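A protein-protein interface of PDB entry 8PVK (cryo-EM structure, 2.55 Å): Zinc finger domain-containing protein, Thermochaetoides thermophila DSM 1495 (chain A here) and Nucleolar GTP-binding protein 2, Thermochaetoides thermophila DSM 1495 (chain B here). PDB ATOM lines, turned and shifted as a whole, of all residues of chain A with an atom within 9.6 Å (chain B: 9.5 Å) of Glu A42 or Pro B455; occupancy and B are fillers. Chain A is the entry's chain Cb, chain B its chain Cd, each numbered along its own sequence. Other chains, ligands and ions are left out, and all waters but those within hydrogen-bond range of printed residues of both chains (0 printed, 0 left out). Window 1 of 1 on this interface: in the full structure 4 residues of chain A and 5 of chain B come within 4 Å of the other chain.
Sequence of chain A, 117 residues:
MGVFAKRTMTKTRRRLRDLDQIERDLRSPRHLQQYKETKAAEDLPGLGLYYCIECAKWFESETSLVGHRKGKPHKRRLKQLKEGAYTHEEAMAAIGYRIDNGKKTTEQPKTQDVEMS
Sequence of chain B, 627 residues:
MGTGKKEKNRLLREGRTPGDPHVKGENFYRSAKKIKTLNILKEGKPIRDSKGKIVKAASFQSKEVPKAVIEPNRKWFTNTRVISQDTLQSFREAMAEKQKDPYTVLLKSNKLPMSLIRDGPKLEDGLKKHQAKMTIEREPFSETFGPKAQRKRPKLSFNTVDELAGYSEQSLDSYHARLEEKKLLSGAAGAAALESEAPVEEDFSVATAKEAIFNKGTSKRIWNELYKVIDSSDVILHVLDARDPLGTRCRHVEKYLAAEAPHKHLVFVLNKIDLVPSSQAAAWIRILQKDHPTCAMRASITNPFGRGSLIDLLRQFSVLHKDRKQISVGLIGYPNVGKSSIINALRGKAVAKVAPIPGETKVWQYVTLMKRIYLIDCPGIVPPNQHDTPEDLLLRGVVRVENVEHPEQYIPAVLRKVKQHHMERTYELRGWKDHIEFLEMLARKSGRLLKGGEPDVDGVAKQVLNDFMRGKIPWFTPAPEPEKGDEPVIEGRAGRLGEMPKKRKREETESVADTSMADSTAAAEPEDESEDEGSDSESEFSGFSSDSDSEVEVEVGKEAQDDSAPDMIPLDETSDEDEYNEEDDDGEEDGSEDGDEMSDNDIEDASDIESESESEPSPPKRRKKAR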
ATOM      1  N   LYS A  36     -24.370 -19.168  -2.163  1.00  0.00           N
ATOM      2  CA  LYS A  36     -23.722 -18.829  -0.902  1.00  0.00           C
ATOM      3  C   LYS A  36     -22.758 -19.912  -0.427  1.00  0.00           C
ATOM      4  O   LYS A  36     -21.759 -19.592   0.225  1.00  0.00           O
ATOM      5  CB  LYS A  36     -24.775 -18.531   0.165  1.00  0.00           C
ATOM      6  CG  LYS A  36     -25.497 -17.214  -0.074  1.00  0.00           C
ATOM      7  CD  LYS A  36     -26.254 -16.741   1.150  1.00  0.00           C
ATOM      8  CE  LYS A  36     -26.828 -15.353   0.923  1.00  0.00           C
ATOM      9  NZ  LYS A  36     -27.534 -14.832   2.124  1.00  0.00           N
ATOM     10  N   LYS A  39     -19.205 -19.584  -1.546  1.00  0.00           N
ATOM     11  CA  LYS A  39     -18.373 -18.570  -0.915  1.00  0.00           C
ATOM     12  C   LYS A  39     -18.045 -18.989   0.512  1.00  0.00           C
ATOM     13  O   LYS A  39     -18.666 -19.893   1.077  1.00  0.00           O
ATOM     14  CB  LYS A  39     -19.060 -17.196  -0.911  1.00  0.00           C
ATOM     15  CG  LYS A  39     -19.383 -16.654  -2.291  1.00  0.00           C
ATOM     16  CD  LYS A  39     -18.111 -16.362  -3.067  1.00  0.00           C
ATOM     17  CE  LYS A  39     -18.411 -15.665  -4.382  1.00  0.00           C
ATOM     18  NZ  LYS A  39     -19.100 -16.570  -5.339  1.00  0.00           N
ATOM     19  N   ALA A  40     -17.054 -18.317   1.091  1.00  0.00           N
ATOM     20  CA  ALA A  40     -16.626 -18.557   2.463  1.00  0.00           C
ATOM     21  C   ALA A  40     -17.167 -17.449   3.355  1.00  0.00           C
ATOM     22  O   ALA A  40     -16.989 -16.265   3.055  1.00  0.00           O
ATOM     23  CB  ALA A  40     -15.100 -18.622   2.562  1.00  0.00           C
ATOM     24  N   ALA A  41     -17.817 -17.839   4.455  1.00  0.00           N
ATOM     25  CA  ALA A  41     -18.503 -16.865   5.299  1.00  0.00           C
ATOM     26  C   ALA A  41     -17.531 -16.006   6.097  1.00  0.00           C
ATOM     27  O   ALA A  41     -17.879 -14.887   6.491  1.00  0.00           O
ATOM     28  CB  ALA A  41     -19.473 -17.577   6.240  1.00  0.00           C
ATOM     29  N   GLU A  42     -16.320 -16.503   6.351  1.00  0.00           N
ATOM     30  CA  GLU A  42     -15.361 -15.737   7.139  1.00  0.00           C
ATOM     31  C   GLU A  42     -14.713 -14.613   6.340  1.00  0.00           C
ATOM     32  O   GLU A  42     -14.136 -13.700   6.939  1.00  0.00           O
ATOM     33  CB  GLU A  42     -14.283 -16.665   7.704  1.00  0.00           C
ATOM     34  CG  GLU A  42     -13.343 -17.245   6.659  1.00  0.00           C
ATOM     35  CD  GLU A  42     -13.801 -18.597   6.146  1.00  0.00           C
ATOM     36  OE1 GLU A  42     -14.959 -18.978   6.418  1.00  0.00           O
ATOM     37  OE2 GLU A  42     -13.002 -19.278   5.471  1.00  0.00           O
ATOM     38  N   ASP A  43     -14.794 -14.655   5.012  1.00  0.00           N
ATOM     39  CA  ASP A  43     -14.200 -13.634   4.161  1.00  0.00           C
ATOM     40  C   ASP A  43     -15.201 -12.582   3.700  1.00  0.00           C
ATOM     41  O   ASP A  43     -14.793 -11.581   3.103  1.00  0.00           O
ATOM     42  CB  ASP A  43     -13.546 -14.287   2.938  1.00  0.00           C
ATOM     43  CG  ASP A  43     -12.320 -15.100   3.300  1.00  0.00           C
ATOM     44  OD1 ASP A  43     -11.910 -15.069   4.478  1.00  0.00           O
ATOM     45  OD2 ASP A  43     -11.767 -15.770   2.404  1.00  0.00           O
ATOM     46  N   LEU A  44     -16.489 -12.779   3.961  1.00  0.00           N
ATOM     47  CA  LEU A  44     -17.533 -11.881   3.491  1.00  0.00           C
ATOM     48  C   LEU A  44     -17.639 -10.650   4.386  1.00  0.00           C
ATOM     49  O   LEU A  44     -17.301 -10.707   5.573  1.00  0.00           O
ATOM     50  CB  LEU A  44     -18.875 -12.606   3.454  1.00  0.00           C
ATOM     51  CG  LEU A  44     -18.985 -13.723   2.417  1.00  0.00           C
ATOM     52  CD1 LEU A  44     -20.283 -14.491   2.586  1.00  0.00           C
ATOM     53  CD2 LEU A  44     -18.868 -13.161   1.011  1.00  0.00           C
ATOM     54  N   PRO A  45     -18.079  -9.519   3.829  1.00  0.00           N
ATOM     55  CA  PRO A  45     -18.349  -8.339   4.664  1.00  0.00           C
ATOM     56  C   PRO A  45     -19.474  -8.610   5.653  1.00  0.00           C
ATOM     57  O   PRO A  45     -20.522  -9.151   5.294  1.00  0.00           O
ATOM     58  CB  PRO A  45     -18.748  -7.264   3.647  1.00  0.00           C
ATOM     59  CG  PRO A  45     -18.219  -7.726   2.346  1.00  0.00           C
ATOM     60  CD  PRO A  45     -18.153  -9.217   2.388  1.00  0.00           C
ATOM     61  N   GLY A  46     -19.250  -8.213   6.904  1.00  0.00           N
ATOM     62  CA  GLY A  46     -20.236  -8.424   7.951  1.00  0.00           C
ATOM     63  C   GLY A  46     -20.510  -9.880   8.256  1.00  0.00           C
ATOM     64  O   GLY A  46     -21.631 -10.222   8.648  1.00  0.00           O
ATOM     65  N   LEU A  47     -19.512 -10.748   8.059  1.00  0.00           N
ATOM     66  CA  LEU A  47     -19.595 -12.200   8.253  1.00  0.00           C
ATOM     67  C   LEU A  47     -20.655 -12.852   7.367  1.00  0.00           C
ATOM     68  O   LEU A  47     -21.134 -13.948   7.676  1.00  0.00           O
ATOM     69  CB  LEU A  47     -19.837 -12.577   9.723  1.00  0.00           C
ATOM     70  CG  LEU A  47     -18.667 -12.658  10.714  1.00  0.00           C
ATOM     71  CD1 LEU A  47     -17.696 -13.761  10.312  1.00  0.00           C
ATOM     72  CD2 LEU A  47     -17.943 -11.330  10.901  1.00  0.00           C
ATOM     73  N   GLY A  48     -21.033 -12.204   6.267  1.00  0.00           N
ATOM     74  CA  GLY A  48     -22.049 -12.736   5.384  1.00  0.00           C
ATOM     75  C   GLY A  48     -23.471 -12.571   5.866  1.00  0.00           C
ATOM     76  O   GLY A  48     -24.389 -13.082   5.215  1.00  0.00           O
ATOM     77  N   LEU A  49     -23.686 -11.872   6.981  1.00  0.00           N
ATOM     78  CA  LEU A  49     -25.018 -11.758   7.559  1.00  0.00           C
ATOM     79  C   LEU A  49     -25.864 -10.679   6.902  1.00  0.00           C
ATOM     80  O   LEU A  49     -27.081 -10.653   7.117  1.00  0.00           O
ATOM     81  CB  LEU A  49     -24.921 -11.475   9.058  1.00  0.00           C
ATOM     82  CG  LEU A  49     -24.113 -12.453   9.910  1.00  0.00           C
ATOM     83  CD1 LEU A  49     -24.272 -12.120  11.382  1.00  0.00           C
ATOM     84  CD2 LEU A  49     -24.541 -13.885   9.635  1.00  0.00           C
ATOM     85  N   TRP A  58     -22.746  -8.103  -0.699  1.00  0.00           N
ATOM     86  CA  TRP A  58     -22.671  -8.147   0.754  1.00  0.00           C
ATOM     87  C   TRP A  58     -22.300  -6.785   1.325  1.00  0.00           C
ATOM     88  O   TRP A  58     -21.693  -5.947   0.651  1.00  0.00           O
ATOM     89  CB  TRP A  58     -21.648  -9.186   1.215  1.00  0.00           C
ATOM     90  CG  TRP A  58     -22.083 -10.615   1.058  1.00  0.00           C
ATOM     91  CD1 TRP A  58     -22.748 -11.374   1.977  1.00  0.00           C
ATOM     92  CD2 TRP A  58     -21.865 -11.462  -0.078  1.00  0.00           C
ATOM     93  NE1 TRP A  58     -22.964 -12.635   1.482  1.00  0.00           N
ATOM     94  CE2 TRP A  58     -22.430 -12.716   0.224  1.00  0.00           C
ATOM     95  CE3 TRP A  58     -21.251 -11.279  -1.319  1.00  0.00           C
ATOM     96  CZ2 TRP A  58     -22.402 -13.782  -0.675  1.00  0.00           C
ATOM     97  CZ3 TRP A  58     -21.222 -12.338  -2.209  1.00  0.00           C
ATOM     98  CH2 TRP A  58     -21.795 -13.573  -1.882  1.00  0.00           C
ATOM     99  N   ILE B 436      -7.646 -19.284  14.956  1.00  0.00           N
ATOM    100  CA  ILE B 436      -8.299 -18.627  13.820  1.00  0.00           C
ATOM    101  C   ILE B 436      -9.215 -17.513  14.304  1.00  0.00           C
ATOM    102  O   ILE B 436      -9.143 -16.372  13.830  1.00  0.00           O
ATOM    103  CB  ILE B 436      -9.087 -19.650  12.981  1.00  0.00           C
ATOM    104  CG1 ILE B 436      -8.181 -20.750  12.428  1.00  0.00           C
ATOM    105  CG2 ILE B 436      -9.857 -18.947  11.862  1.00  0.00           C
ATOM    106  CD1 ILE B 436      -7.416 -20.334  11.212  1.00  0.00           C
ATOM    107  N   GLU B 437     -10.076 -17.825  15.274  1.00  0.00           N
ATOM    108  CA  GLU B 437     -11.018 -16.832  15.772  1.00  0.00           C
ATOM    109  C   GLU B 437     -10.315 -15.752  16.583  1.00  0.00           C
ATOM    110  O   GLU B 437     -10.746 -14.594  16.563  1.00  0.00           O
ATOM    111  CB  GLU B 437     -12.104 -17.513  16.600  1.00  0.00           C
ATOM    112  CG  GLU B 437     -13.360 -16.683  16.756  1.00  0.00           C
ATOM    113  CD  GLU B 437     -14.341 -17.296  17.727  1.00  0.00           C
ATOM    114  OE1 GLU B 437     -13.984 -18.301  18.370  1.00  0.00           O
ATOM    115  OE2 GLU B 437     -15.480 -16.798  17.823  1.00  0.00           O
ATOM    116  N   PHE B 438      -9.239 -16.108  17.293  1.00  0.00           N
ATOM    117  CA  PHE B 438      -8.452 -15.109  18.014  1.00  0.00           C
ATOM    118  C   PHE B 438      -7.857 -14.081  17.057  1.00  0.00           C
ATOM    119  O   PHE B 438      -7.976 -12.867  17.277  1.00  0.00           O
ATOM    120  CB  PHE B 438      -7.352 -15.803  18.825  1.00  0.00           C
ATOM    121  CG  PHE B 438      -6.220 -14.894  19.227  1.00  0.00           C
ATOM    122  CD1 PHE B 438      -6.368 -13.999  20.276  1.00  0.00           C
ATOM    123  CD2 PHE B 438      -4.999 -14.950  18.569  1.00  0.00           C
ATOM    124  CE1 PHE B 438      -5.328 -13.167  20.649  1.00  0.00           C
ATOM    125  CE2 PHE B 438      -3.959 -14.119  18.936  1.00  0.00           C
ATOM    126  CZ  PHE B 438      -4.123 -13.228  19.978  1.00  0.00           C
ATOM    127  N   LEU B 439      -7.242 -14.552  15.967  1.00  0.00           N
ATOM    128  CA  LEU B 439      -6.670 -13.632  14.991  1.00  0.00           C
ATOM    129  C   LEU B 439      -7.747 -12.842  14.258  1.00  0.00           C
ATOM    130  O   LEU B 439      -7.538 -11.665  13.946  1.00  0.00           O
ATOM    131  CB  LEU B 439      -5.795 -14.393  13.995  1.00  0.00           C
ATOM    132  CG  LEU B 439      -4.550 -15.073  14.574  1.00  0.00           C
ATOM    133  CD1 LEU B 439      -3.910 -15.974  13.540  1.00  0.00           C
ATOM    134  CD2 LEU B 439      -3.546 -14.070  15.110  1.00  0.00           C
ATOM    135  N   GLU B 440      -8.905 -13.459  13.993  1.00  0.00           N
ATOM    136  CA  GLU B 440      -9.994 -12.743  13.330  1.00  0.00           C
ATOM    137  C   GLU B 440     -10.553 -11.626  14.206  1.00  0.00           C
ATOM    138  O   GLU B 440     -10.791 -10.513  13.720  1.00  0.00           O
ATOM    139  CB  GLU B 440     -11.099 -13.720  12.934  1.00  0.00           C
ATOM    140  CG  GLU B 440     -10.799 -14.512  11.673  1.00  0.00           C
ATOM    141  CD  GLU B 440     -11.713 -15.708  11.501  1.00  0.00           C
ATOM    142  OE1 GLU B 440     -12.512 -15.986  12.419  1.00  0.00           O
ATOM    143  OE2 GLU B 440     -11.632 -16.375  10.446  1.00  0.00           O
ATOM    144  N   MET B 441     -10.767 -11.901  15.498  1.00  0.00           N
ATOM    145  CA  MET B 441     -11.229 -10.857  16.408  1.00  0.00           C
ATOM    146  C   MET B 441     -10.190  -9.760  16.581  1.00  0.00           C
ATOM    147  O   MET B 441     -10.546  -8.580  16.672  1.00  0.00           O
ATOM    148  CB  MET B 441     -11.604 -11.440  17.769  1.00  0.00           C
ATOM    149  CG  MET B 441     -12.817 -12.336  17.782  1.00  0.00           C
ATOM    150  SD  MET B 441     -13.126 -12.944  19.448  1.00  0.00           S
ATOM    151  CE  MET B 441     -14.520 -14.016  19.153  1.00  0.00           C
ATOM    152  N   LEU B 442      -8.904 -10.122  16.638  1.00  0.00           N
ATOM    153  CA  LEU B 442      -7.866  -9.100  16.755  1.00  0.00           C
ATOM    154  C   LEU B 442      -7.813  -8.217  15.511  1.00  0.00           C
ATOM    155  O   LEU B 442      -7.664  -6.994  15.620  1.00  0.00           O
ATOM    156  CB  LEU B 442      -6.511  -9.755  17.018  1.00  0.00           C
ATOM    157  CG  LEU B 442      -5.363  -8.838  17.448  1.00  0.00           C
ATOM    158  CD1 LEU B 442      -5.833  -7.761  18.418  1.00  0.00           C
ATOM    159  CD2 LEU B 442      -4.240  -9.654  18.064  1.00  0.00           C
ATOM    160  N   ALA B 443      -7.956  -8.818  14.324  1.00  0.00           N
ATOM    161  CA  ALA B 443      -7.983  -8.043  13.088  1.00  0.00           C
ATOM    162  C   ALA B 443      -9.200  -7.130  13.022  1.00  0.00           C
ATOM    163  O   ALA B 443      -9.090  -5.973  12.603  1.00  0.00           O
ATOM    164  CB  ALA B 443      -7.962  -8.980  11.883  1.00  0.00           C
ATOM    165  N   ARG B 444     -10.368  -7.631  13.433  1.00  0.00           N
ATOM    166  CA  ARG B 444     -11.570  -6.806  13.408  1.00  0.00           C
ATOM    167  C   ARG B 444     -11.506  -5.682  14.432  1.00  0.00           C
ATOM    168  O   ARG B 444     -12.029  -4.590  14.183  1.00  0.00           O
ATOM    169  CB  ARG B 444     -12.809  -7.671  13.640  1.00  0.00           C
ATOM    170  CG  ARG B 444     -13.479  -8.135  12.357  1.00  0.00           C
ATOM    171  CD  ARG B 444     -14.791  -8.848  12.636  1.00  0.00           C
ATOM    172  NE  ARG B 444     -14.634  -9.934  13.595  1.00  0.00           N
ATOM    173  CZ  ARG B 444     -14.604 -11.220  13.272  1.00  0.00           C
ATOM    174  NH1 ARG B 444     -14.707 -11.620  12.016  1.00  0.00           N
ATOM    175  NH2 ARG B 444     -14.463 -12.128  14.235  1.00  0.00           N
ATOM    176  N   LYS B 445     -10.876  -5.923  15.583  1.00  0.00           N
ATOM    177  CA  LYS B 445     -10.751  -4.876  16.589  1.00  0.00           C
ATOM    178  C   LYS B 445      -9.742  -3.814  16.169  1.00  0.00           C
ATOM    179  O   LYS B 445      -9.971  -2.618  16.379  1.00  0.00           O
ATOM    180  CB  LYS B 445     -10.352  -5.483  17.931  1.00  0.00           C
ATOM    181  CG  LYS B 445     -10.385  -4.496  19.079  1.00  0.00           C
ATOM    182  CD  LYS B 445      -9.839  -5.118  20.343  1.00  0.00           C
ATOM    183  CE  LYS B 445      -8.356  -5.387  20.193  1.00  0.00           C
ATOM    184  NZ  LYS B 445      -7.575  -4.131  20.029  1.00  0.00           N
ATOM    185  N   SER B 446      -8.627  -4.227  15.570  1.00  0.00           N
ATOM    186  CA  SER B 446      -7.564  -3.298  15.214  1.00  0.00           C
ATOM    187  C   SER B 446      -7.674  -2.773  13.789  1.00  0.00           C
ATOM    188  O   SER B 446      -6.784  -2.039  13.349  1.00  0.00           O
ATOM    189  CB  SER B 446      -6.201  -3.965  15.419  1.00  0.00           C
ATOM    190  OG  SER B 446      -6.157  -5.234  14.793  1.00  0.00           O
ATOM    191  N   GLY B 447      -8.732  -3.125  13.061  1.00  0.00           N
ATOM    192  CA  GLY B 447      -8.898  -2.604  11.719  1.00  0.00           C
ATOM    193  C   GLY B 447      -7.968  -3.199  10.690  1.00  0.00           C
ATOM    194  O   GLY B 447      -7.684  -2.554   9.678  1.00  0.00           O
ATOM    195  N   ARG B 448      -7.475  -4.415  10.923  1.00  0.00           N
ATOM    196  CA  ARG B 448      -6.583  -5.093   9.987  1.00  0.00           C
ATOM    197  C   ARG B 448      -7.442  -5.786   8.933  1.00  0.00           C
ATOM    198  O   ARG B 448      -7.650  -7.003   8.946  1.00  0.00           O
ATOM    199  CB  ARG B 448      -5.686  -6.078  10.722  1.00  0.00           C
ATOM    200  CG  ARG B 448      -4.775  -5.456  11.777  1.00  0.00           C
ATOM    201  CD  ARG B 448      -3.708  -4.591  11.148  1.00  0.00           C
ATOM    202  NE  ARG B 448      -4.104  -3.190  11.119  1.00  0.00           N
ATOM    203  CZ  ARG B 448      -3.706  -2.327  10.198  1.00  0.00           C
ATOM    204  NH1 ARG B 448      -2.921  -2.697   9.203  1.00  0.00           N
ATOM    205  NH2 ARG B 448      -4.121  -1.067  10.266  1.00  0.00           N
ATOM    206  N   LEU B 449      -7.950  -4.986   8.003  1.00  0.00           N
ATOM    207  CA  LEU B 449      -8.923  -5.440   7.021  1.00  0.00           C
ATOM    208  C   LEU B 449      -8.366  -5.289   5.614  1.00  0.00           C
ATOM    209  O   LEU B 449      -7.704  -4.296   5.299  1.00  0.00           O
ATOM    210  CB  LEU B 449     -10.232  -4.657   7.144  1.00  0.00           C
ATOM    211  CG  LEU B 449     -10.774  -4.477   8.561  1.00  0.00           C
ATOM    212  CD1 LEU B 449     -11.898  -3.454   8.573  1.00  0.00           C
ATOM    213  CD2 LEU B 449     -11.239  -5.807   9.131  1.00  0.00           C
ATOM    214  N   LEU B 450      -8.641  -6.281   4.775  1.00  0.00           N
ATOM    215  CA  LEU B 450      -8.299  -6.228   3.364  1.00  0.00           C
ATOM    216  C   LEU B 450      -9.472  -5.625   2.592  1.00  0.00           C
ATOM    217  O   LEU B 450     -10.399  -5.059   3.177  1.00  0.00           O
ATOM    218  CB  LEU B 450      -7.927  -7.621   2.858  1.00  0.00           C
ATOM    219  CG  LEU B 450      -6.706  -8.265   3.516  1.00  0.00           C
ATOM    220  CD1 LEU B 450      -6.502  -9.679   3.002  1.00  0.00           C
ATOM    221  CD2 LEU B 450      -5.464  -7.422   3.278  1.00  0.00           C
ATOM    222  N   LYS B 451      -9.439  -5.731   1.266  1.00  0.00           N
ATOM    223  CA  LYS B 451     -10.534  -5.225   0.450  1.00  0.00           C
ATOM    224  C   LYS B 451     -11.777  -6.082   0.650  1.00  0.00           C
ATOM    225  O   LYS B 451     -11.724  -7.310   0.545  1.00  0.00           O
ATOM    226  CB  LYS B 451     -10.133  -5.199  -1.023  1.00  0.00           C
ATOM    227  CG  LYS B 451      -9.040  -4.196  -1.337  1.00  0.00           C
ATOM    228  CD  LYS B 451      -9.471  -2.789  -0.966  1.00  0.00           C
ATOM    229  CE  LYS B 451      -8.415  -1.766  -1.348  1.00  0.00           C
ATOM    230  NZ  LYS B 451      -8.805  -0.393  -0.925  1.00  0.00           N
ATOM    231  N   GLY B 452     -12.898  -5.428   0.936  1.00  0.00           N
ATOM    232  CA  GLY B 452     -14.115  -6.122   1.291  1.00  0.00           C
ATOM    233  C   GLY B 452     -14.281  -6.409   2.765  1.00  0.00           C
ATOM    234  O   GLY B 452     -15.143  -7.218   3.126  1.00  0.00           O
ATOM    235  N   GLY B 453     -13.476  -5.793   3.628  1.00  0.00           N
ATOM    236  CA  GLY B 453     -13.608  -6.008   5.054  1.00  0.00           C
ATOM    237  C   GLY B 453     -13.109  -7.342   5.558  1.00  0.00           C
ATOM    238  O   GLY B 453     -13.353  -7.677   6.721  1.00  0.00           O
ATOM    239  N   GLU B 454     -12.431  -8.116   4.720  1.00  0.00           N
ATOM    240  CA  GLU B 454     -11.910  -9.409   5.146  1.00  0.00           C
ATOM    241  C   GLU B 454     -10.731  -9.206   6.093  1.00  0.00           C
ATOM    242  O   GLU B 454      -9.864  -8.368   5.818  1.00  0.00           O
ATOM    243  CB  GLU B 454     -11.491 -10.232   3.930  1.00  0.00           C
ATOM    244  CG  GLU B 454     -10.695 -11.484   4.252  1.00  0.00           C
ATOM    245  CD  GLU B 454      -9.965 -12.035   3.045  1.00  0.00           C
ATOM    246  OE1 GLU B 454     -10.093 -11.445   1.953  1.00  0.00           O
ATOM    247  OE2 GLU B 454      -9.264 -13.058   3.189  1.00  0.00           O
ATOM    248  N   PRO B 455     -10.678  -9.922   7.216  1.00  0.00           N
ATOM    249  CA  PRO B 455      -9.572  -9.740   8.164  1.00  0.00           C
ATOM    250  C   PRO B 455      -8.225 -10.153   7.588  1.00  0.00           C
ATOM    251  O   PRO B 455      -8.121 -11.081   6.783  1.00  0.00           O
ATOM    252  CB  PRO B 455      -9.967 -10.644   9.341  1.00  0.00           C
ATOM    253  CG  PRO B 455     -10.958 -11.606   8.778  1.00  0.00           C
ATOM    254  CD  PRO B 455     -11.701 -10.845   7.734  1.00  0.00           C
ATOM    255  N   ASP B 456      -7.182  -9.440   8.018  1.00  0.00           N
ATOM    256  CA  ASP B 456      -5.811  -9.713   7.583  1.00  0.00           C
ATOM    257  C   ASP B 456      -5.157 -10.623   8.620  1.00  0.00           C
ATOM    258  O   ASP B 456      -4.388 -10.195   9.489  1.00  0.00           O
ATOM    259  CB  ASP B 456      -5.038  -8.415   7.388  1.00  0.00           C
ATOM    260  CG  ASP B 456      -3.719  -8.620   6.670  1.00  0.00           C
ATOM    261  OD1 ASP B 456      -3.444  -9.755   6.227  1.00  0.00           O
ATOM    262  OD2 ASP B 456      -2.955  -7.641   6.543  1.00  0.00           O
ATOM    263  N   VAL B 457      -5.473 -11.914   8.498  1.00  0.00           N
ATOM    264  CA  VAL B 457      -5.077 -12.905   9.494  1.00  0.00           C
ATOM    265  C   VAL B 457      -3.562 -13.079   9.519  1.00  0.00           C
ATOM    266  O   VAL B 457      -2.957 -13.175  10.592  1.00  0.00           O
ATOM    267  CB  VAL B 457      -5.809 -14.232   9.220  1.00  0.00           C
ATOM    268  CG1 VAL B 457      -5.398 -15.297  10.210  1.00  0.00           C
ATOM    269  CG2 VAL B 457      -7.312 -14.019   9.268  1.00  0.00           C
ATOM    270  N   ASP B 458      -2.923 -13.093   8.346  1.00  0.00           N
ATOM    271  CA  ASP B 458      -1.473 -13.270   8.287  1.00  0.00           C
ATOM    272  C   ASP B 458      -0.733 -12.064   8.861  1.00  0.00           C
ATOM    273  O   ASP B 458       0.276 -12.224   9.559  1.00  0.00           O
ATOM    274  CB  ASP B 458      -1.039 -13.534   6.847  1.00  0.00           C
ATOM    275  CG  ASP B 458      -0.934 -15.014   6.533  1.00  0.00           C
ATOM    276  OD1 ASP B 458      -1.295 -15.835   7.402  1.00  0.00           O
ATOM    277  OD2 ASP B 458      -0.497 -15.358   5.415  1.00  0.00           O
ATOM    278  N   GLY B 459      -1.222 -10.854   8.585  1.00  0.00           N
ATOM    279  CA  GLY B 459      -0.604  -9.669   9.156  1.00  0.00           C
ATOM    280  C   GLY B 459      -0.766  -9.591  10.663  1.00  0.00           C
ATOM    281  O   GLY B 459       0.165  -9.201  11.379  1.00  0.00           O
ATOM    282  N   VAL B 460      -1.941  -9.976  11.167  1.00  0.00           N
ATOM    283  CA  VAL B 460      -2.146 -10.016  12.612  1.00  0.00           C
ATOM    284  C   VAL B 460      -1.269 -11.089  13.249  1.00  0.00           C
ATOM    285  O   VAL B 460      -0.735 -10.899  14.347  1.00  0.00           O
ATOM    286  CB  VAL B 460      -3.640 -10.216  12.926  1.00  0.00           C
ATOM    287  CG1 VAL B 460      -3.874 -10.470  14.400  1.00  0.00           C
ATOM    288  CG2 VAL B 460      -4.388  -8.994  12.524  1.00  0.00           C
ATOM    289  N   ALA B 461      -1.079 -12.215  12.555  1.00  0.00           N
ATOM    290  CA  ALA B 461      -0.185 -13.255  13.052  1.00  0.00           C
ATOM    291  C   ALA B 461       1.254 -12.760  13.126  1.00  0.00           C
ATOM    292  O   ALA B 461       1.965 -13.047  14.096  1.00  0.00           O
ATOM    293  CB  ALA B 461      -0.279 -14.495  12.164  1.00  0.00           C
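Of the 26 printed residues of chain B, 5 touch a printed residue of chain A. Printed residues of chain B that touch a printed residue of chain A: Glu B440, Arg B444, Gly B452, Glu B454 and Pro B455. Hydrophobic or aromatic side chains of chain B that line the printed part of chain A: Pro B455. Printed residues of chain A that touch a printed residue of chain B: Glu A42, Asp A43, Pro A45 and Leu A47. Hydrophobic or aromatic side chains of chain A within 4 Å of the printed part of chain B: Pro A45 and Leu A47. Along chain A the printed residues that touch a printed residue of chain B span positions 42 to 47. Among the printed residues, no Asp or Glu carboxylate lies within 4 Å of a Lys or Arg side-chain nitrogen of the other chain.
Glu A42 touches just these residues of chain B: Glu B440 and Pro B455. Pro B455 touches one residue of chain A. Asp A43 touches one residue of chain B. Glu B440 touches just one residue of chain A: Glu A42 (3.8 Å). Of the printed residues of chain A, Arg B444 touches Leu A47 (3.4 Å). Of the printed residues of chain A, Gly B452 touches Pro A45 (3.2 Å). Of the printed residues of chain B, Pro A45 touches Gly B452 (3.2 Å). Printed residues of chain B within 4 Å of Leu A47: Arg B444. The nearest residue of chain A that does not touch Pro B455 is Asp A43 (5.2 Å). The nearest printed residue of chain A that does not touch Gly B452 is Asp A43 (4.4 Å).
Among the printed residues, merely in contact across the chains: Glu A42 with Glu B440 (3.8 Å), Glu A42 with Pro B455 (3.8 Å), Asp A43 with Glu B454 (3.6 Å), Pro A45 with Gly B452 (3.2 Å) and Leu A47 with Arg B444 (3.4 Å).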
